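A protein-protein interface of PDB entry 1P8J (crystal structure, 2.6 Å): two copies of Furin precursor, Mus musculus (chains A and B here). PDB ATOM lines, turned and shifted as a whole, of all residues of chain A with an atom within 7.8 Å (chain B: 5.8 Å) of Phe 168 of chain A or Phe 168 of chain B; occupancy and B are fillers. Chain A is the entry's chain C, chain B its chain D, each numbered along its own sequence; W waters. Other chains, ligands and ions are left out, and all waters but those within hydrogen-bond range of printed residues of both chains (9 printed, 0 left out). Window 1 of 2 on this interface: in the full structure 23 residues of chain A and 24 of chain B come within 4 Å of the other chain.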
ATOM      1  N   LEU A 162      21.693 -32.711   8.333  1.00  0.00           N
ATOM      2  CA  LEU A 162      20.733 -31.750   8.873  1.00  0.00           C
ATOM      3  C   LEU A 162      20.043 -32.229  10.136  1.00  0.00           C
ATOM      4  O   LEU A 162      19.783 -31.443  11.040  1.00  0.00           O
ATOM      5  CB  LEU A 162      19.682 -31.380   7.821  1.00  0.00           C
ATOM      6  CG  LEU A 162      20.161 -30.521   6.639  1.00  0.00           C
ATOM      7  CD1 LEU A 162      18.985 -30.180   5.764  1.00  0.00           C
ATOM      8  CD2 LEU A 162      20.824 -29.241   7.126  1.00  0.00           C
ATOM      9  N   ALA A 163      19.732 -33.512  10.207  1.00  0.00           N
ATOM     10  CA  ALA A 163      19.088 -34.046  11.396  1.00  0.00           C
ATOM     11  C   ALA A 163      20.068 -33.988  12.577  1.00  0.00           C
ATOM     12  O   ALA A 163      19.681 -33.694  13.708  1.00  0.00           O
ATOM     13  CB  ALA A 163      18.651 -35.474  11.150  1.00  0.00           C
ATOM     14  N   GLU A 164      21.339 -34.277  12.312  1.00  0.00           N
ATOM     15  CA  GLU A 164      22.344 -34.246  13.360  1.00  0.00           C
ATOM     16  C   GLU A 164      22.419 -32.829  13.891  1.00  0.00           C
ATOM     17  O   GLU A 164      22.544 -32.617  15.094  1.00  0.00           O
ATOM     18  CB  GLU A 164      23.717 -34.658  12.832  1.00  0.00           C
ATOM     19  CG  GLU A 164      24.752 -34.819  13.937  1.00  0.00           C
ATOM     20  CD  GLU A 164      24.506 -36.058  14.789  1.00  0.00           C
ATOM     21  OE1 GLU A 164      24.833 -36.051  16.001  1.00  0.00           O
ATOM     22  OE2 GLU A 164      23.991 -37.052  14.235  1.00  0.00           O
ATOM     23  N   GLU A 165      22.353 -31.860  12.984  1.00  0.00           N
ATOM     24  CA  GLU A 165      22.390 -30.462  13.377  1.00  0.00           C
ATOM     25  C   GLU A 165      21.147 -30.148  14.200  1.00  0.00           C
ATOM     26  O   GLU A 165      21.225 -29.512  15.241  1.00  0.00           O
ATOM     27  CB  GLU A 165      22.444 -29.544  12.146  1.00  0.00           C
ATOM     28  CG  GLU A 165      23.840 -29.371  11.550  1.00  0.00           C
ATOM     29  CD  GLU A 165      23.876 -28.375  10.392  1.00  0.00           C
ATOM     30  OE1 GLU A 165      24.984 -27.958   9.989  1.00  0.00           O
ATOM     31  OE2 GLU A 165      22.803 -28.008   9.875  1.00  0.00           O
ATOM     32  N   ALA A 166      19.995 -30.600  13.732  1.00  0.00           N
ATOM     33  CA  ALA A 166      18.753 -30.357  14.446  1.00  0.00           C
ATOM     34  C   ALA A 166      18.837 -30.837  15.887  1.00  0.00           C
ATOM     35  O   ALA A 166      18.429 -30.132  16.805  1.00  0.00           O
ATOM     36  CB  ALA A 166      17.615 -31.047  13.740  1.00  0.00           C
ATOM     37  N   PHE A 167      19.361 -32.040  16.081  1.00  0.00           N
ATOM     38  CA  PHE A 167      19.491 -32.605  17.411  1.00  0.00           C
ATOM     39  C   PHE A 167      20.319 -31.714  18.320  1.00  0.00           C
ATOM     40  O   PHE A 167      19.898 -31.381  19.425  1.00  0.00           O
ATOM     41  CB  PHE A 167      20.143 -33.988  17.343  1.00  0.00           C
ATOM     42  CG  PHE A 167      19.168 -35.115  17.204  1.00  0.00           C
ATOM     43  CD1 PHE A 167      19.406 -36.140  16.305  1.00  0.00           C
ATOM     44  CD2 PHE A 167      18.044 -35.185  18.011  1.00  0.00           C
ATOM     45  CE1 PHE A 167      18.544 -37.226  16.217  1.00  0.00           C
ATOM     46  CE2 PHE A 167      17.172 -36.262  17.932  1.00  0.00           C
ATOM     47  CZ  PHE A 167      17.422 -37.287  17.036  1.00  0.00           C
ATOM     48  N   PHE A 168      21.502 -31.321  17.865  1.00  0.00           N
ATOM     49  CA  PHE A 168      22.346 -30.505  18.711  1.00  0.00           C
ATOM     50  C   PHE A 168      21.777 -29.115  18.894  1.00  0.00           C
ATOM     51  O   PHE A 168      21.872 -28.537  19.972  1.00  0.00           O
ATOM     52  CB  PHE A 168      23.770 -30.434  18.167  1.00  0.00           C
ATOM     53  CG  PHE A 168      24.741 -29.796  19.125  1.00  0.00           C
ATOM     54  CD1 PHE A 168      25.068 -28.447  19.016  1.00  0.00           C
ATOM     55  CD2 PHE A 168      25.279 -30.529  20.170  1.00  0.00           C
ATOM     56  CE1 PHE A 168      25.916 -27.839  19.937  1.00  0.00           C
ATOM     57  CE2 PHE A 168      26.128 -29.934  21.100  1.00  0.00           C
ATOM     58  CZ  PHE A 168      26.447 -28.589  20.986  1.00  0.00           C
ATOM     59  N   ARG A 169      21.171 -28.590  17.842  1.00  0.00           N
ATOM     60  CA  ARG A 169      20.576 -27.268  17.891  1.00  0.00           C
ATOM     61  C   ARG A 169      19.447 -27.244  18.911  1.00  0.00           C
ATOM     62  O   ARG A 169      19.326 -26.308  19.704  1.00  0.00           O
ATOM     63  CB  ARG A 169      20.013 -26.900  16.522  1.00  0.00           C
ATOM     64  CG  ARG A 169      19.517 -25.473  16.414  1.00  0.00           C
ATOM     65  CD  ARG A 169      18.784 -25.251  15.099  1.00  0.00           C
ATOM     66  NE  ARG A 169      18.447 -23.844  14.897  1.00  0.00           N
ATOM     67  CZ  ARG A 169      19.338 -22.889  14.616  1.00  0.00           C
ATOM     68  NH1 ARG A 169      18.922 -21.630  14.459  1.00  0.00           N
ATOM     69  NH2 ARG A 169      20.639 -23.186  14.480  1.00  0.00           N
ATOM     70  N   GLY A 170      18.620 -28.281  18.891  1.00  0.00           N
ATOM     71  CA  GLY A 170      17.500 -28.327  19.805  1.00  0.00           C
ATOM     72  C   GLY A 170      17.906 -28.502  21.251  1.00  0.00           C
ATOM     73  O   GLY A 170      17.278 -27.970  22.165  1.00  0.00           O
ATOM     74  N   VAL A 171      18.968 -29.258  21.455  1.00  0.00           N
ATOM     75  CA  VAL A 171      19.462 -29.545  22.783  1.00  0.00           C
ATOM     76  C   VAL A 171      20.178 -28.319  23.351  1.00  0.00           C
ATOM     77  O   VAL A 171      20.272 -28.155  24.567  1.00  0.00           O
ATOM     78  CB  VAL A 171      20.394 -30.780  22.719  1.00  0.00           C
ATOM     79  CG1 VAL A 171      21.720 -30.479  23.358  1.00  0.00           C
ATOM     80  CG2 VAL A 171      19.723 -31.969  23.364  1.00  0.00           C
ATOM     81  N   SER A 172      20.652 -27.450  22.463  1.00  0.00           N
ATOM     82  CA  SER A 172      21.367 -26.236  22.857  1.00  0.00           C
ATOM     83  C   SER A 172      20.480 -25.004  22.996  1.00  0.00           C
ATOM     84  O   SER A 172      20.603 -24.239  23.953  1.00  0.00           O
ATOM     85  CB  SER A 172      22.444 -25.902  21.831  1.00  0.00           C
ATOM     86  OG  SER A 172      23.378 -26.956  21.728  1.00  0.00           O
ATOM     87  N   GLN A 173      19.590 -24.818  22.028  1.00  0.00           N
ATOM     88  CA  GLN A 173      18.723 -23.655  22.002  1.00  0.00           C
ATOM     89  C   GLN A 173      17.247 -23.892  22.318  1.00  0.00           C
ATOM     90  O   GLN A 173      16.515 -22.947  22.597  1.00  0.00           O
ATOM     91  CB  GLN A 173      18.852 -22.999  20.632  1.00  0.00           C
ATOM     92  CG  GLN A 173      20.257 -22.508  20.322  1.00  0.00           C
ATOM     93  CD  GLN A 173      20.506 -22.308  18.821  1.00  0.00           C
ATOM     94  OE1 GLN A 173      19.595 -21.927  18.062  1.00  0.00           O
ATOM     95  NE2 GLN A 173      21.747 -22.552  18.392  1.00  0.00           N
ATOM     96  N   GLY A 174      16.803 -25.139  22.266  1.00  0.00           N
ATOM     97  CA  GLY A 174      15.403 -25.419  22.539  1.00  0.00           C
ATOM     98  C   GLY A 174      15.002 -25.026  23.940  1.00  0.00           C
ATOM     99  O   GLY A 174      15.852 -24.909  24.814  1.00  0.00           O
ATOM    100  N   GLY A 179      17.121 -26.835  26.456  1.00  0.00           N
ATOM    101  CA  GLY A 179      17.266 -27.991  25.589  1.00  0.00           C
ATOM    102  C   GLY A 179      16.010 -28.804  25.340  1.00  0.00           C
ATOM    103  O   GLY A 179      15.300 -29.167  26.274  1.00  0.00           O
ATOM    104  N   SER A 180      15.729 -29.094  24.073  1.00  0.00           N
ATOM    105  CA  SER A 180      14.566 -29.894  23.720  1.00  0.00           C
ATOM    106  C   SER A 180      14.787 -31.287  24.295  1.00  0.00           C
ATOM    107  O   SER A 180      15.922 -31.750  24.415  1.00  0.00           O
ATOM    108  CB  SER A 180      14.429 -30.029  22.201  1.00  0.00           C
ATOM    109  OG  SER A 180      14.312 -28.778  21.564  1.00  0.00           O
ATOM    110  N   PHE A 182      14.196 -35.088  23.609  1.00  0.00           N
ATOM    111  CA  PHE A 182      13.848 -36.057  22.587  1.00  0.00           C
ATOM    112  C   PHE A 182      13.736 -37.454  23.161  1.00  0.00           C
ATOM    113  O   PHE A 182      14.737 -38.041  23.556  1.00  0.00           O
ATOM    114  CB  PHE A 182      14.906 -36.054  21.495  1.00  0.00           C
ATOM    115  CG  PHE A 182      15.099 -34.718  20.835  1.00  0.00           C
ATOM    116  CD1 PHE A 182      16.278 -33.995  21.019  1.00  0.00           C
ATOM    117  CD2 PHE A 182      14.127 -34.205  19.977  1.00  0.00           C
ATOM    118  CE1 PHE A 182      16.492 -32.776  20.346  1.00  0.00           C
ATOM    119  CE2 PHE A 182      14.332 -32.988  19.302  1.00  0.00           C
ATOM    120  CZ  PHE A 182      15.515 -32.277  19.485  1.00  0.00           C
ATOM    121  N   SER A 204      21.958 -41.997  20.030  1.00  0.00           N
ATOM    122  CA  SER A 204      22.360 -40.604  20.223  1.00  0.00           C
ATOM    123  C   SER A 204      22.337 -40.209  21.699  1.00  0.00           C
ATOM    124  O   SER A 204      21.518 -40.718  22.471  1.00  0.00           O
ATOM    125  CB  SER A 204      21.415 -39.677  19.458  1.00  0.00           C
ATOM    126  OG  SER A 204      21.783 -38.314  19.634  1.00  0.00           O
ATOM    127  N   ILE A 205      23.217 -39.294  22.100  1.00  0.00           N
ATOM    128  CA  ILE A 205      23.211 -38.880  23.497  1.00  0.00           C
ATOM    129  C   ILE A 205      22.100 -37.856  23.700  1.00  0.00           C
ATOM    130  O   ILE A 205      21.682 -37.589  24.829  1.00  0.00           O
ATOM    131  CB  ILE A 205      24.544 -38.237  23.942  1.00  0.00           C
ATOM    132  CG1 ILE A 205      24.706 -36.862  23.301  1.00  0.00           C
ATOM    133  CG2 ILE A 205      25.711 -39.128  23.567  1.00  0.00           C
ATOM    134  CD1 ILE A 205      25.889 -36.097  23.847  1.00  0.00           C
ATOM    135  N   TYR A 206      21.608 -37.297  22.600  1.00  0.00           N
ATOM    136  CA  TYR A 206      20.567 -36.275  22.666  1.00  0.00           C
ATOM    137  C   TYR A 206      19.184 -36.838  22.877  1.00  0.00           C
ATOM    138  O   TYR A 206      18.234 -36.087  23.053  1.00  0.00           O
ATOM    139  CB  TYR A 206      20.542 -35.442  21.385  1.00  0.00           C
ATOM    140  CG  TYR A 206      21.889 -34.920  20.971  1.00  0.00           C
ATOM    141  CD1 TYR A 206      22.451 -35.282  19.745  1.00  0.00           C
ATOM    142  CD2 TYR A 206      22.613 -34.070  21.805  1.00  0.00           C
ATOM    143  CE1 TYR A 206      23.706 -34.809  19.359  1.00  0.00           C
ATOM    144  CE2 TYR A 206      23.867 -33.587  21.430  1.00  0.00           C
ATOM    145  CZ  TYR A 206      24.411 -33.960  20.210  1.00  0.00           C
ATOM    146  OH  TYR A 206      25.662 -33.492  19.855  1.00  0.00           O
ATOM    147  N   TRP A 283      18.035 -30.554  29.414  1.00  0.00           N
ATOM    148  CA  TRP A 283      17.916 -31.857  28.756  1.00  0.00           C
ATOM    149  C   TRP A 283      18.794 -32.890  29.463  1.00  0.00           C
ATOM    150  O   TRP A 283      18.463 -34.068  29.492  1.00  0.00           O
ATOM    151  CB  TRP A 283      18.286 -31.757  27.267  1.00  0.00           C
ATOM    152  CG  TRP A 283      19.739 -31.446  26.969  1.00  0.00           C
ATOM    153  CD1 TRP A 283      20.343 -30.214  26.968  1.00  0.00           C
ATOM    154  CD2 TRP A 283      20.758 -32.392  26.603  1.00  0.00           C
ATOM    155  NE1 TRP A 283      21.670 -30.338  26.621  1.00  0.00           N
ATOM    156  CE2 TRP A 283      21.952 -31.662  26.396  1.00  0.00           C
ATOM    157  CE3 TRP A 283      20.775 -33.785  26.433  1.00  0.00           C
ATOM    158  CZ2 TRP A 283      23.149 -32.279  26.026  1.00  0.00           C
ATOM    159  CZ3 TRP A 283      21.969 -34.394  26.065  1.00  0.00           C
ATOM    160  CH2 TRP A 283      23.140 -33.638  25.866  1.00  0.00           C
ATOM    161  N   GLN A 340      28.575 -29.269  30.892  1.00  0.00           N
ATOM    162  CA  GLN A 340      29.026 -30.503  30.270  1.00  0.00           C
ATOM    163  C   GLN A 340      30.418 -30.404  29.688  1.00  0.00           C
ATOM    164  O   GLN A 340      30.712 -29.504  28.910  1.00  0.00           O
ATOM    165  CB  GLN A 340      28.055 -30.903  29.161  1.00  0.00           C
ATOM    166  CG  GLN A 340      28.428 -32.168  28.408  1.00  0.00           C
ATOM    167  CD  GLN A 340      27.759 -32.236  27.040  1.00  0.00           C
ATOM    168  OE1 GLN A 340      27.979 -31.366  26.189  1.00  0.00           O
ATOM    169  NE2 GLN A 340      26.933 -33.264  26.824  1.00  0.00           N
ATOM    170  N   LYS A 342      33.557 -32.397  27.534  1.00  0.00           N
ATOM    171  CA  LYS A 342      33.679 -33.388  26.469  1.00  0.00           C
ATOM    172  C   LYS A 342      35.142 -33.728  26.315  1.00  0.00           C
ATOM    173  O   LYS A 342      35.927 -32.910  25.858  1.00  0.00           O
ATOM    174  CB  LYS A 342      33.144 -32.818  25.158  1.00  0.00           C
ATOM    175  CG  LYS A 342      33.154 -33.790  23.995  1.00  0.00           C
ATOM    176  CD  LYS A 342      32.643 -33.102  22.745  1.00  0.00           C
ATOM    177  CE  LYS A 342      32.549 -34.056  21.582  1.00  0.00           C
ATOM    178  NZ  LYS A 342      31.885 -33.412  20.418  1.00  0.00           N
ATOM    179  N   TYR A 464      31.763 -37.843  28.047  1.00  0.00           N
ATOM    180  CA  TYR A 464      30.947 -36.682  28.365  1.00  0.00           C
ATOM    181  C   TYR A 464      30.740 -36.729  29.877  1.00  0.00           C
ATOM    182  O   TYR A 464      30.626 -37.807  30.456  1.00  0.00           O
ATOM    183  CB  TYR A 464      29.604 -36.769  27.650  1.00  0.00           C
ATOM    184  CG  TYR A 464      29.661 -36.407  26.186  1.00  0.00           C
ATOM    185  CD1 TYR A 464      29.616 -35.076  25.776  1.00  0.00           C
ATOM    186  CD2 TYR A 464      29.752 -37.396  25.209  1.00  0.00           C
ATOM    187  CE1 TYR A 464      29.651 -34.733  24.427  1.00  0.00           C
ATOM    188  CE2 TYR A 464      29.791 -37.070  23.854  1.00  0.00           C
ATOM    189  CZ  TYR A 464      29.733 -35.734  23.471  1.00  0.00           C
ATOM    190  OH  TYR A 464      29.699 -35.394  22.131  1.00  0.00           O
ATOM    191  N   ALA B 163      35.034 -32.826  14.201  1.00  0.00           N
ATOM    192  CA  ALA B 163      35.384 -31.433  13.953  1.00  0.00           C
ATOM    193  C   ALA B 163      34.101 -30.627  13.741  1.00  0.00           C
ATOM    194  O   ALA B 163      33.976 -29.496  14.206  1.00  0.00           O
ATOM    195  CB  ALA B 163      36.280 -31.335  12.736  1.00  0.00           C
ATOM    196  N   GLU B 164      33.140 -31.213  13.036  1.00  0.00           N
ATOM    197  CA  GLU B 164      31.887 -30.527  12.798  1.00  0.00           C
ATOM    198  C   GLU B 164      31.245 -30.222  14.148  1.00  0.00           C
ATOM    199  O   GLU B 164      30.729 -29.123  14.365  1.00  0.00           O
ATOM    200  CB  GLU B 164      30.949 -31.387  11.948  1.00  0.00           C
ATOM    201  CG  GLU B 164      29.693 -30.630  11.527  1.00  0.00           C
ATOM    202  CD  GLU B 164      29.997 -29.519  10.544  1.00  0.00           C
ATOM    203  OE1 GLU B 164      29.282 -28.495  10.522  1.00  0.00           O
ATOM    204  OE2 GLU B 164      30.964 -29.689   9.777  1.00  0.00           O
ATOM    205  N   GLU B 165      31.280 -31.199  15.051  1.00  0.00           N
ATOM    206  CA  GLU B 165      30.719 -31.031  16.384  1.00  0.00           C
ATOM    207  C   GLU B 165      31.475 -29.916  17.110  1.00  0.00           C
ATOM    208  O   GLU B 165      30.874 -29.043  17.735  1.00  0.00           O
ATOM    209  CB  GLU B 165      30.823 -32.339  17.192  1.00  0.00           C
ATOM    210  CG  GLU B 165      29.683 -33.342  16.942  1.00  0.00           C
ATOM    211  CD  GLU B 165      29.750 -34.586  17.844  1.00  0.00           C
ATOM    212  OE1 GLU B 165      28.776 -35.381  17.865  1.00  0.00           O
ATOM    213  OE2 GLU B 165      30.774 -34.781  18.528  1.00  0.00           O
ATOM    214  N   ALA B 166      32.799 -29.939  17.008  1.00  0.00           N
ATOM    215  CA  ALA B 166      33.625 -28.939  17.668  1.00  0.00           C
ATOM    216  C   ALA B 166      33.233 -27.521  17.250  1.00  0.00           C
ATOM    217  O   ALA B 166      33.116 -26.620  18.090  1.00  0.00           O
ATOM    218  CB  ALA B 166      35.086 -29.194  17.359  1.00  0.00           C
ATOM    219  N   PHE B 167      33.033 -27.331  15.952  1.00  0.00           N
ATOM    220  CA  PHE B 167      32.662 -26.029  15.428  1.00  0.00           C
ATOM    221  C   PHE B 167      31.359 -25.555  16.034  1.00  0.00           C
ATOM    222  O   PHE B 167      31.259 -24.434  16.502  1.00  0.00           O
ATOM    223  CB  PHE B 167      32.495 -26.097  13.910  1.00  0.00           C
ATOM    224  CG  PHE B 167      33.745 -25.803  13.142  1.00  0.00           C
ATOM    225  CD1 PHE B 167      34.153 -26.642  12.112  1.00  0.00           C
ATOM    226  CD2 PHE B 167      34.492 -24.664  13.416  1.00  0.00           C
ATOM    227  CE1 PHE B 167      35.292 -26.349  11.364  1.00  0.00           C
ATOM    228  CE2 PHE B 167      35.630 -24.363  12.675  1.00  0.00           C
ATOM    229  CZ  PHE B 167      36.032 -25.210  11.643  1.00  0.00           C
ATOM    230  N   PHE B 168      30.350 -26.415  16.011  1.00  0.00           N
ATOM    231  CA  PHE B 168      29.050 -26.046  16.534  1.00  0.00           C
ATOM    232  C   PHE B 168      29.098 -25.860  18.050  1.00  0.00           C
ATOM    233  O   PHE B 168      28.488 -24.944  18.600  1.00  0.00           O
ATOM    234  CB  PHE B 168      28.042 -27.124  16.140  1.00  0.00           C
ATOM    235  CG  PHE B 168      26.623 -26.641  16.107  1.00  0.00           C
ATOM    236  CD1 PHE B 168      25.606 -27.475  15.642  1.00  0.00           C
ATOM    237  CD2 PHE B 168      26.297 -25.361  16.549  1.00  0.00           C
ATOM    238  CE1 PHE B 168      24.286 -27.039  15.621  1.00  0.00           C
ATOM    239  CE2 PHE B 168      24.988 -24.916  16.533  1.00  0.00           C
ATOM    240  CZ  PHE B 168      23.979 -25.753  16.070  1.00  0.00           C
ATOM    241  N   ARG B 169      29.840 -26.736  18.713  1.00  0.00           N
ATOM    242  CA  ARG B 169      29.978 -26.683  20.152  1.00  0.00           C
ATOM    243  C   ARG B 169      30.654 -25.385  20.567  1.00  0.00           C
ATOM    244  O   ARG B 169      30.223 -24.728  21.519  1.00  0.00           O
ATOM    245  CB  ARG B 169      30.815 -27.869  20.626  1.00  0.00           C
ATOM    246  CG  ARG B 169      30.885 -28.034  22.132  1.00  0.00           C
ATOM    247  CD  ARG B 169      31.836 -29.163  22.512  1.00  0.00           C
ATOM    248  NE  ARG B 169      31.832 -29.428  23.950  1.00  0.00           N
ATOM    249  CZ  ARG B 169      30.830 -30.022  24.591  1.00  0.00           C
ATOM    250  NH1 ARG B 169      30.902 -30.217  25.901  1.00  0.00           N
ATOM    251  NH2 ARG B 169      29.761 -30.434  23.915  1.00  0.00           N
ATOM    252  N   GLY B 170      31.708 -25.014  19.849  1.00  0.00           N
ATOM    253  CA  GLY B 170      32.442 -23.811  20.189  1.00  0.00           C
ATOM    254  C   GLY B 170      31.666 -22.534  19.957  1.00  0.00           C
ATOM    255  O   GLY B 170      31.806 -21.551  20.696  1.00  0.00           O
ATOM    256  N   VAL B 171      30.835 -22.558  18.928  1.00  0.00           N
ATOM    257  CA  VAL B 171      30.035 -21.412  18.550  1.00  0.00           C
ATOM    258  C   VAL B 171      28.860 -21.235  19.505  1.00  0.00           C
ATOM    259  O   VAL B 171      28.339 -20.128  19.666  1.00  0.00           O
ATOM    260  CB  VAL B 171      29.557 -21.601  17.086  1.00  0.00           C
ATOM    261  CG1 VAL B 171      28.052 -21.417  16.964  1.00  0.00           C
ATOM    262  CG2 VAL B 171      30.324 -20.658  16.183  1.00  0.00           C
ATOM    263  N   SER B 172      28.461 -22.328  20.153  1.00  0.00           N
ATOM    264  CA  SER B 172      27.342 -22.307  21.088  1.00  0.00           C
ATOM    265  C   SER B 172      27.748 -22.113  22.531  1.00  0.00           C
ATOM    266  O   SER B 172      27.078 -21.398  23.270  1.00  0.00           O
ATOM    267  CB  SER B 172      26.566 -23.616  21.032  1.00  0.00           C
ATOM    268  OG  SER B 172      26.178 -23.925  19.713  1.00  0.00           O
ATOM    269  N   GLN B 173      28.837 -22.756  22.930  1.00  0.00           N
ATOM    270  CA  GLN B 173      29.282 -22.712  24.312  1.00  0.00           C
ATOM    271  C   GLN B 173      30.563 -21.952  24.588  1.00  0.00           C
ATOM    272  O   GLN B 173      30.841 -21.596  25.740  1.00  0.00           O
ATOM    273  CB  GLN B 173      29.425 -24.144  24.813  1.00  0.00           C
ATOM    274  CG  GLN B 173      28.114 -24.909  24.749  1.00  0.00           C
ATOM    275  CD  GLN B 173      28.301 -26.406  24.871  1.00  0.00           C
ATOM    276  OE1 GLN B 173      29.306 -26.881  25.428  1.00  0.00           O
ATOM    277  NE2 GLN B 173      27.328 -27.166  24.363  1.00  0.00           N
ATOM    278  N   TYR B 206      30.362 -21.137  10.540  1.00  0.00           N
ATOM    279  CA  TYR B 206      30.994 -20.899  11.833  1.00  0.00           C
ATOM    280  C   TYR B 206      32.337 -20.201  11.726  1.00  0.00           C
ATOM    281  O   TYR B 206      32.916 -19.824  12.740  1.00  0.00           O
ATOM    282  CB  TYR B 206      31.208 -22.221  12.575  1.00  0.00           C
ATOM    283  CG  TYR B 206      29.987 -23.111  12.637  1.00  0.00           C
ATOM    284  CD1 TYR B 206      30.011 -24.405  12.101  1.00  0.00           C
ATOM    285  CD2 TYR B 206      28.806 -22.664  13.225  1.00  0.00           C
ATOM    286  CE1 TYR B 206      28.881 -25.226  12.153  1.00  0.00           C
ATOM    287  CE2 TYR B 206      27.675 -23.473  13.283  1.00  0.00           C
ATOM    288  CZ  TYR B 206      27.720 -24.749  12.744  1.00  0.00           C
ATOM    289  OH  TYR B 206      26.589 -25.529  12.769  1.00  0.00           O
HETATM  290  O   HOH W   1      26.986 -28.218  11.619  1.00  0.00           O
HETATM  291  O   HOH W   2      29.498 -31.852  21.144  1.00  0.00           O
HETATM  292  O   HOH W   3      26.291 -29.397  24.683  1.00  0.00           O
HETATM  293  O   HOH W   4      34.043 -32.361  19.113  1.00  0.00           O
HETATM  294  O   HOH W   5      30.587 -36.775  20.260  1.00  0.00           O
HETATM  295  O   HOH W   6      28.629 -27.009  27.890  1.00  0.00           O
HETATM  296  O   HOH W   7      25.994 -25.096   9.448  1.00  0.00           O
HETATM  297  O   HOH W   8      27.586 -36.762  20.523  1.00  0.00           O
HETATM  298  O   HOH W   9      26.544 -34.164  17.426  1.00  0.00           O
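The side-chain amide oxygen of Gln 340 of chain A lies within hydrogen-bond range of the guanidinium group of Arg 169 of chain B (3.0 Å). The side-chain carboxylate (OE2) of Glu 165 of chain B lies within salt-bridge range of the side-chain amino group (NZ) of Lys 342 of chain A (2.6 Å).
Glu 165 of chain A touches Phe 168 of chain B, but with the chains exchanged Phe 168 of chain A does not touch Glu 165 of chain B (5.5 Å). Phe 168 of chain B touches its own counterpart, Phe 168 of chain A. Phe 168 of chain A touches Ser 172 of chain B, but with the chains exchanged Ser 172 of chain A does not touch Phe 168 of chain B (5.8 Å). Phe 168 of chain A touches Gln 173 of chain B, but with the chains exchanged Gln 173 of chain A does not touch Phe 168 of chain B (4.4 Å). Of the 8 pairs that touch across the chains among the printed residues, 1 has its exchanged pair printed and touching as well.
Water W3 lies within hydrogen-bond range of the side-chain amide nitrogen (NE2) of Gln 173 of chain B (2.5 Å) and the side-chain amide oxygen (OE1) of Gln 340 of chain A (3.0 Å). Water W5 lies within hydrogen-bond range of the side-chain hydroxyl (OH) of Tyr 464 of chain A (2.5 Å) and the side-chain carboxylate (OE2) of Glu 165 of chain B (2.6 Å). Water W1 lies within hydrogen-bond range of OE1 of Glu 164 of chain B (2.6 Å), OE1 of Glu 165 of chain A (2.6 Å) and OH of Tyr 206 of chain B (3.0 Å). Water W9 lies within hydrogen-bond range of OE1 of Glu 165 of chain B (2.6 Å), OH of Tyr 206 of chain A (2.7 Å) and OE1 of Glu 164 of chain A (2.9 Å). Water W8 lies within hydrogen-bond range of OH of Tyr 464 of chain A (3.0 Å) and OE1 of Glu 165 of chain B (3.2 Å). Water W7 bridges the side-chain carboxylate (OE1) of Glu 165 of chain A (3.1 Å) and the side-chain hydroxyl (OH) of Tyr 206 of chain B (3.4 Å).
Among the printed residues, merely in contact across the chains: Glu 165 of chain A with Phe 168 of chain B (3.95 Å), Phe 168 of chain A with Phe 168 of chain B (3.6 Å), Phe 168 of chain A with Ser 172 of chain B (3.9 Å), Phe 168 of chain A with Gln 173 of chain B (3.8 Å), Lys 342 of chain A with Arg 169 of chain B (3.5 Å) and Tyr 464 of chain A with Glu 165 of chain B (3.8 Å).
Of the 23 printed residues of chain A, 5 touch a printed residue of chain B. Printed residues of chain A that touch a printed residue of chain B: Glu 165, Phe 168, Gln 340, Lys 342 and Tyr 464. Hydrophobic or aromatic side chains of chain B that line the printed part of chain A: Phe 168.
The side-chain hydroxyl (OG) of Ser 172 of chain B is in hydrogen-bond range of the backbone carbonyl oxygen (O) of Phe 168 of chain B. The backbone carbonyl oxygen of Phe 168 of chain A is in hydrogen-bond range of the side-chain hydroxyl of Ser 172 of chain A (2.8 Å). OH of Tyr 464 of chain A sits close to NZ of Lys 342 of chain A (3.4 Å).
Ser 204 of chain A touches none of the printed residues of chain B. Of the printed residues of chain B, Lys 342 of chain A touches Glu 165 and Arg 169. Printed residues of chain B within 4 Å of Tyr 464 of chain A: Glu 165. Of the printed residues of chain A, Glu 165 of chain B touches Lys 342 (2.6 Å) and Tyr 464 (3.8 Å). Phe 167 of chain B touches none of the printed residues of chain A. Of the printed residues of chain A, Phe 168 of chain B touches Glu 165 and Phe 168. The nearest residue of chain A that does not touch Phe 168 of chain B is Arg 169 of chain A (4.1 Å).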
